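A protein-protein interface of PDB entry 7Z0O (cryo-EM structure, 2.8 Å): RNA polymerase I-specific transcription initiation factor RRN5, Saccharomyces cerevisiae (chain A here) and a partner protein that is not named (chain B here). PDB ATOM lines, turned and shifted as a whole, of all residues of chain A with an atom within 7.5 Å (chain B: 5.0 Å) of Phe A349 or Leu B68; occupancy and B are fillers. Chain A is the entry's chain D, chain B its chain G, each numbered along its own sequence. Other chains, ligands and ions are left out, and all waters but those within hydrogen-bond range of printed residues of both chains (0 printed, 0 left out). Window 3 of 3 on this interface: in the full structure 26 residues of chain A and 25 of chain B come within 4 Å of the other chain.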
ATOM      1  N   TYR A 126      10.063  20.606   1.210  1.00  0.00           N
ATOM      2  CA  TYR A 126       9.610  20.723   2.586  1.00  0.00           C
ATOM      3  C   TYR A 126       8.305  19.969   2.787  1.00  0.00           C
ATOM      4  O   TYR A 126       7.328  20.191   2.066  1.00  0.00           O
ATOM      5  CB  TYR A 126       9.449  22.194   2.959  1.00  0.00           C
ATOM      6  CG  TYR A 126      10.713  22.985   2.744  1.00  0.00           C
ATOM      7  CD1 TYR A 126      11.776  22.877   3.626  1.00  0.00           C
ATOM      8  CD2 TYR A 126      10.851  23.824   1.651  1.00  0.00           C
ATOM      9  CE1 TYR A 126      12.936  23.589   3.431  1.00  0.00           C
ATOM     10  CE2 TYR A 126      12.008  24.542   1.447  1.00  0.00           C
ATOM     11  CZ  TYR A 126      13.048  24.420   2.341  1.00  0.00           C
ATOM     12  OH  TYR A 126      14.207  25.132   2.148  1.00  0.00           O
ATOM     13  N   ILE A 343      19.031  12.734   9.872  1.00  0.00           N
ATOM     14  CA  ILE A 343      18.706  13.501   8.674  1.00  0.00           C
ATOM     15  C   ILE A 343      17.214  13.803   8.626  1.00  0.00           C
ATOM     16  O   ILE A 343      16.801  14.911   8.265  1.00  0.00           O
ATOM     17  CB  ILE A 343      19.173  12.752   7.414  1.00  0.00           C
ATOM     18  CG1 ILE A 343      20.686  12.538   7.450  1.00  0.00           C
ATOM     19  CG2 ILE A 343      18.785  13.515   6.164  1.00  0.00           C
ATOM     20  CD1 ILE A 343      21.483  13.816   7.347  1.00  0.00           C
ATOM     21  N   ASP A 344      16.382  12.825   8.989  1.00  0.00           N
ATOM     22  CA  ASP A 344      14.937  13.027   8.961  1.00  0.00           C
ATOM     23  C   ASP A 344      14.500  14.095   9.956  1.00  0.00           C
ATOM     24  O   ASP A 344      13.649  14.932   9.638  1.00  0.00           O
ATOM     25  CB  ASP A 344      14.219  11.709   9.241  1.00  0.00           C
ATOM     26  CG  ASP A 344      12.775  11.727   8.788  1.00  0.00           C
ATOM     27  OD1 ASP A 344      12.501  12.252   7.690  1.00  0.00           O
ATOM     28  OD2 ASP A 344      11.911  11.217   9.532  1.00  0.00           O
ATOM     29  N   GLU A 345      15.065  14.081  11.168  1.00  0.00           N
ATOM     30  CA  GLU A 345      14.680  15.076  12.165  1.00  0.00           C
ATOM     31  C   GLU A 345      15.069  16.481  11.726  1.00  0.00           C
ATOM     32  O   GLU A 345      14.318  17.437  11.954  1.00  0.00           O
ATOM     33  CB  GLU A 345      15.305  14.750  13.521  1.00  0.00           C
ATOM     34  CG  GLU A 345      14.533  13.724  14.332  1.00  0.00           C
ATOM     35  CD  GLU A 345      15.259  12.401  14.447  1.00  0.00           C
ATOM     36  OE1 GLU A 345      16.468  12.360  14.148  1.00  0.00           O
ATOM     37  OE2 GLU A 345      14.620  11.401  14.837  1.00  0.00           O
ATOM     38  N   ALA A 346      16.242  16.629  11.108  1.00  0.00           N
ATOM     39  CA  ALA A 346      16.647  17.937  10.605  1.00  0.00           C
ATOM     40  C   ALA A 346      15.705  18.423   9.511  1.00  0.00           C
ATOM     41  O   ALA A 346      15.334  19.602   9.480  1.00  0.00           O
ATOM     42  CB  ALA A 346      18.084  17.879  10.089  1.00  0.00           C
ATOM     43  N   ASP A 347      15.308  17.527   8.605  1.00  0.00           N
ATOM     44  CA  ASP A 347      14.387  17.911   7.541  1.00  0.00           C
ATOM     45  C   ASP A 347      13.014  18.262   8.096  1.00  0.00           C
ATOM     46  O   ASP A 347      12.351  19.176   7.594  1.00  0.00           O
ATOM     47  CB  ASP A 347      14.279  16.789   6.510  1.00  0.00           C
ATOM     48  CG  ASP A 347      15.529  16.655   5.664  1.00  0.00           C
ATOM     49  OD1 ASP A 347      16.553  17.279   6.012  1.00  0.00           O
ATOM     50  OD2 ASP A 347      15.488  15.926   4.650  1.00  0.00           O
ATOM     51  N   LEU A 348      12.564  17.540   9.124  1.00  0.00           N
ATOM     52  CA  LEU A 348      11.285  17.864   9.746  1.00  0.00           C
ATOM     53  C   LEU A 348      11.317  19.247  10.381  1.00  0.00           C
ATOM     54  O   LEU A 348      10.346  20.005  10.285  1.00  0.00           O
ATOM     55  CB  LEU A 348      10.922  16.808  10.787  1.00  0.00           C
ATOM     56  CG  LEU A 348      10.402  15.473  10.256  1.00  0.00           C
ATOM     57  CD1 LEU A 348      10.109  14.524  11.405  1.00  0.00           C
ATOM     58  CD2 LEU A 348       9.166  15.681   9.399  1.00  0.00           C
ATOM     59  N   PHE A 349      12.424  19.590  11.043  1.00  0.00           N
ATOM     60  CA  PHE A 349      12.537  20.906  11.662  1.00  0.00           C
ATOM     61  C   PHE A 349      12.569  22.012  10.615  1.00  0.00           C
ATOM     62  O   PHE A 349      11.922  23.051  10.785  1.00  0.00           O
ATOM     63  CB  PHE A 349      13.784  20.965  12.542  1.00  0.00           C
ATOM     64  CG  PHE A 349      13.853  22.186  13.409  1.00  0.00           C
ATOM     65  CD1 PHE A 349      13.296  22.182  14.675  1.00  0.00           C
ATOM     66  CD2 PHE A 349      14.471  23.339  12.960  1.00  0.00           C
ATOM     67  CE1 PHE A 349      13.355  23.302  15.475  1.00  0.00           C
ATOM     68  CE2 PHE A 349      14.533  24.462  13.755  1.00  0.00           C
ATOM     69  CZ  PHE A 349      13.975  24.444  15.014  1.00  0.00           C
ATOM     70  N   ARG A 350      13.319  21.813   9.531  1.00  0.00           N
ATOM     71  CA  ARG A 350      13.377  22.824   8.481  1.00  0.00           C
ATOM     72  C   ARG A 350      12.022  23.000   7.813  1.00  0.00           C
ATOM     73  O   ARG A 350      11.628  24.122   7.475  1.00  0.00           O
ATOM     74  CB  ARG A 350      14.441  22.455   7.451  1.00  0.00           C
ATOM     75  CG  ARG A 350      15.859  22.555   7.969  1.00  0.00           C
ATOM     76  CD  ARG A 350      16.841  21.959   6.984  1.00  0.00           C
ATOM     77  NE  ARG A 350      16.784  22.632   5.692  1.00  0.00           N
ATOM     78  CZ  ARG A 350      17.295  22.143   4.572  1.00  0.00           C
ATOM     79  NH1 ARG A 350      17.902  20.969   4.544  1.00  0.00           N
ATOM     80  NH2 ARG A 350      17.195  22.852   3.450  1.00  0.00           N
ATOM     81  N   SER A 351      11.299  21.899   7.600  1.00  0.00           N
ATOM     82  CA  SER A 351       9.965  21.992   7.019  1.00  0.00           C
ATOM     83  C   SER A 351       9.008  22.729   7.946  1.00  0.00           C
ATOM     84  O   SER A 351       8.187  23.531   7.488  1.00  0.00           O
ATOM     85  CB  SER A 351       9.435  20.596   6.702  1.00  0.00           C
ATOM     86  OG  SER A 351      10.266  19.937   5.765  1.00  0.00           O
ATOM     87  N   ALA A 352       9.091  22.464   9.252  1.00  0.00           N
ATOM     88  CA  ALA A 352       8.225  23.153  10.202  1.00  0.00           C
ATOM     89  C   ALA A 352       8.518  24.645  10.230  1.00  0.00           C
ATOM     90  O   ALA A 352       7.598  25.466  10.325  1.00  0.00           O
ATOM     91  CB  ALA A 352       8.385  22.548  11.594  1.00  0.00           C
ATOM     92  N   LEU A 353       9.796  25.017  10.163  1.00  0.00           N
ATOM     93  CA  LEU A 353      10.153  26.429  10.097  1.00  0.00           C
ATOM     94  C   LEU A 353       9.701  27.054   8.784  1.00  0.00           C
ATOM     95  O   LEU A 353       9.213  28.189   8.768  1.00  0.00           O
ATOM     96  CB  LEU A 353      11.658  26.597  10.281  1.00  0.00           C
ATOM     97  CG  LEU A 353      12.155  28.039  10.339  1.00  0.00           C
ATOM     98  CD1 LEU A 353      11.501  28.766  11.497  1.00  0.00           C
ATOM     99  CD2 LEU A 353      13.666  28.079  10.459  1.00  0.00           C
ATOM    100  N   HIS A 354       9.857  26.329   7.674  1.00  0.00           N
ATOM    101  CA  HIS A 354       9.445  26.858   6.378  1.00  0.00           C
ATOM    102  C   HIS A 354       7.946  27.117   6.340  1.00  0.00           C
ATOM    103  O   HIS A 354       7.499  28.149   5.828  1.00  0.00           O
ATOM    104  CB  HIS A 354       9.852  25.892   5.268  1.00  0.00           C
ATOM    105  CG  HIS A 354       9.458  26.346   3.898  1.00  0.00           C
ATOM    106  ND1 HIS A 354       8.216  26.094   3.359  1.00  0.00           N
ATOM    107  CD2 HIS A 354      10.143  27.034   2.956  1.00  0.00           C
ATOM    108  CE1 HIS A 354       8.152  26.608   2.145  1.00  0.00           C
ATOM    109  NE2 HIS A 354       9.309  27.185   1.877  1.00  0.00           N
ATOM    110  N   GLU A 355       7.153  26.189   6.875  1.00  0.00           N
ATOM    111  CA  GLU A 355       5.715  26.408   6.961  1.00  0.00           C
ATOM    112  C   GLU A 355       5.394  27.573   7.886  1.00  0.00           C
ATOM    113  O   GLU A 355       4.454  28.335   7.637  1.00  0.00           O
ATOM    114  CB  GLU A 355       5.023  25.133   7.440  1.00  0.00           C
ATOM    115  CG  GLU A 355       3.513  25.182   7.390  1.00  0.00           C
ATOM    116  CD  GLU A 355       2.881  23.950   8.002  1.00  0.00           C
ATOM    117  OE1 GLU A 355       3.469  22.857   7.880  1.00  0.00           O
ATOM    118  OE2 GLU A 355       1.796  24.075   8.607  1.00  0.00           O
ATOM    119  N   ARG B  66      13.232  28.326  19.533  1.00  0.00           N
ATOM    120  CA  ARG B  66      12.060  27.514  19.817  1.00  0.00           C
ATOM    121  C   ARG B  66      12.228  26.144  19.180  1.00  0.00           C
ATOM    122  O   ARG B  66      12.672  26.033  18.033  1.00  0.00           O
ATOM    123  CB  ARG B  66      10.777  28.183  19.314  1.00  0.00           C
ATOM    124  CG  ARG B  66      10.880  28.779  17.924  1.00  0.00           C
ATOM    125  CD  ARG B  66       9.608  29.527  17.568  1.00  0.00           C
ATOM    126  NE  ARG B  66       9.717  30.227  16.295  1.00  0.00           N
ATOM    127  CZ  ARG B  66       8.718  30.876  15.713  1.00  0.00           C
ATOM    128  NH1 ARG B  66       7.517  30.932  16.264  1.00  0.00           N
ATOM    129  NH2 ARG B  66       8.928  31.482  14.548  1.00  0.00           N
ATOM    130  N   SER B  67      11.876  25.107  19.932  1.00  0.00           N
ATOM    131  CA  SER B  67      12.069  23.736  19.494  1.00  0.00           C
ATOM    132  C   SER B  67      11.034  23.361  18.436  1.00  0.00           C
ATOM    133  O   SER B  67      10.209  24.174  18.011  1.00  0.00           O
ATOM    134  CB  SER B  67      11.999  22.787  20.687  1.00  0.00           C
ATOM    135  OG  SER B  67      10.657  22.440  20.983  1.00  0.00           O
ATOM    136  N   LEU B  68      11.087  22.102  18.001  1.00  0.00           N
ATOM    137  CA  LEU B  68      10.138  21.620  17.004  1.00  0.00           C
ATOM    138  C   LEU B  68       8.716  21.614  17.552  1.00  0.00           C
ATOM    139  O   LEU B  68       7.765  21.918  16.824  1.00  0.00           O
ATOM    140  CB  LEU B  68      10.540  20.223  16.534  1.00  0.00           C
ATOM    141  CG  LEU B  68       9.577  19.502  15.591  1.00  0.00           C
ATOM    142  CD1 LEU B  68       9.326  20.334  14.346  1.00  0.00           C
ATOM    143  CD2 LEU B  68      10.118  18.132  15.222  1.00  0.00           C
ATOM    144  N   GLU B  69       8.553  21.270  18.831  1.00  0.00           N
ATOM    145  CA  GLU B  69       7.220  21.221  19.423  1.00  0.00           C
ATOM    146  C   GLU B  69       6.553  22.590  19.382  1.00  0.00           C
ATOM    147  O   GLU B  69       5.387  22.699  18.987  1.00  0.00           O
ATOM    148  CB  GLU B  69       7.322  20.707  20.865  1.00  0.00           C
ATOM    149  CG  GLU B  69       6.210  21.070  21.888  1.00  0.00           C
ATOM    150  CD  GLU B  69       4.759  21.011  21.386  1.00  0.00           C
ATOM    151  OE1 GLU B  69       3.862  21.342  22.190  1.00  0.00           O
ATOM    152  OE2 GLU B  69       4.486  20.552  20.257  1.00  0.00           O
ATOM    153  N   ASP B  70       7.282  23.647  19.749  1.00  0.00           N
ATOM    154  CA  ASP B  70       6.703  24.985  19.736  1.00  0.00           C
ATOM    155  C   ASP B  70       6.304  25.403  18.326  1.00  0.00           C
ATOM    156  O   ASP B  70       5.264  26.041  18.131  1.00  0.00           O
ATOM    157  CB  ASP B  70       7.686  25.989  20.334  1.00  0.00           C
ATOM    158  CG  ASP B  70       8.457  25.421  21.505  1.00  0.00           C
ATOM    159  OD1 ASP B  70       7.892  25.357  22.616  1.00  0.00           O
ATOM    160  OD2 ASP B  70       9.629  25.034  21.315  1.00  0.00           O
ATOM    161  N   LEU B  71       7.125  25.062  17.332  1.00  0.00           N
ATOM    162  CA  LEU B  71       6.782  25.384  15.951  1.00  0.00           C
ATOM    163  C   LEU B  71       5.521  24.653  15.510  1.00  0.00           C
ATOM    164  O   LEU B  71       4.663  25.234  14.836  1.00  0.00           O
ATOM    165  CB  LEU B  71       7.949  25.038  15.027  1.00  0.00           C
ATOM    166  CG  LEU B  71       9.070  26.070  14.932  1.00  0.00           C
ATOM    167  CD1 LEU B  71      10.078  25.667  13.871  1.00  0.00           C
ATOM    168  CD2 LEU B  71       8.503  27.445  14.638  1.00  0.00           C
ATOM    169  N   LEU B  72       5.391  23.377  15.878  1.00  0.00           N
ATOM    170  CA  LEU B  72       4.251  22.587  15.425  1.00  0.00           C
ATOM    171  C   LEU B  72       2.941  23.123  15.988  1.00  0.00           C
ATOM    172  O   LEU B  72       1.946  23.244  15.267  1.00  0.00           O
ATOM    173  CB  LEU B  72       4.440  21.121  15.810  1.00  0.00           C
ATOM    174  CG  LEU B  72       5.526  20.350  15.061  1.00  0.00           C
ATOM    175  CD1 LEU B  72       5.562  18.904  15.522  1.00  0.00           C
ATOM    176  CD2 LEU B  72       5.307  20.435  13.562  1.00  0.00           C
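Of chain A, only Phe A349 and Ala A352 come within 4 Å of Leu B68.
Of the printed residues of chain B, Leu A353 touches Leu B71.
Printed residues of chain A within 4 Å of Arg B66: Phe A349 (3.7 Å).
Of the printed residues of chain A, Ser B67 touches Phe A349 (3.8 Å).
Asp B70 touches none of the printed residues of chain A.
Glu B69 touches none of the printed residues of chain A.
The nearest printed residue of chain B that does not touch Leu A353 is Arg B66 (4.8 Å).
Phe A349 touches Arg B66.
Phe A349 touches Ser B67.
Leu B68 touches Phe A349.
Ala A352 touches Leu B68.
Leu B71 touches Leu A353 (CD1 to N, 3.8 Å).
Hydrophobic or aromatic side chains of chain B that line the printed part of chain A: Leu B68 and Leu B71.
Of the 14 printed residues of chain A, 3 touch a printed residue of chain B.
Among the printed residues, 5 pairs touch across the chains.
N of Glu B69 lies within hydrogen-bond range of OG of Ser B67 (3.2 Å).
The side-chain carboxylate (OD2) of Asp B70 sits at hydrogen-bond distance from the backbone NH (N) of Ser B67, 2.6 Å away.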
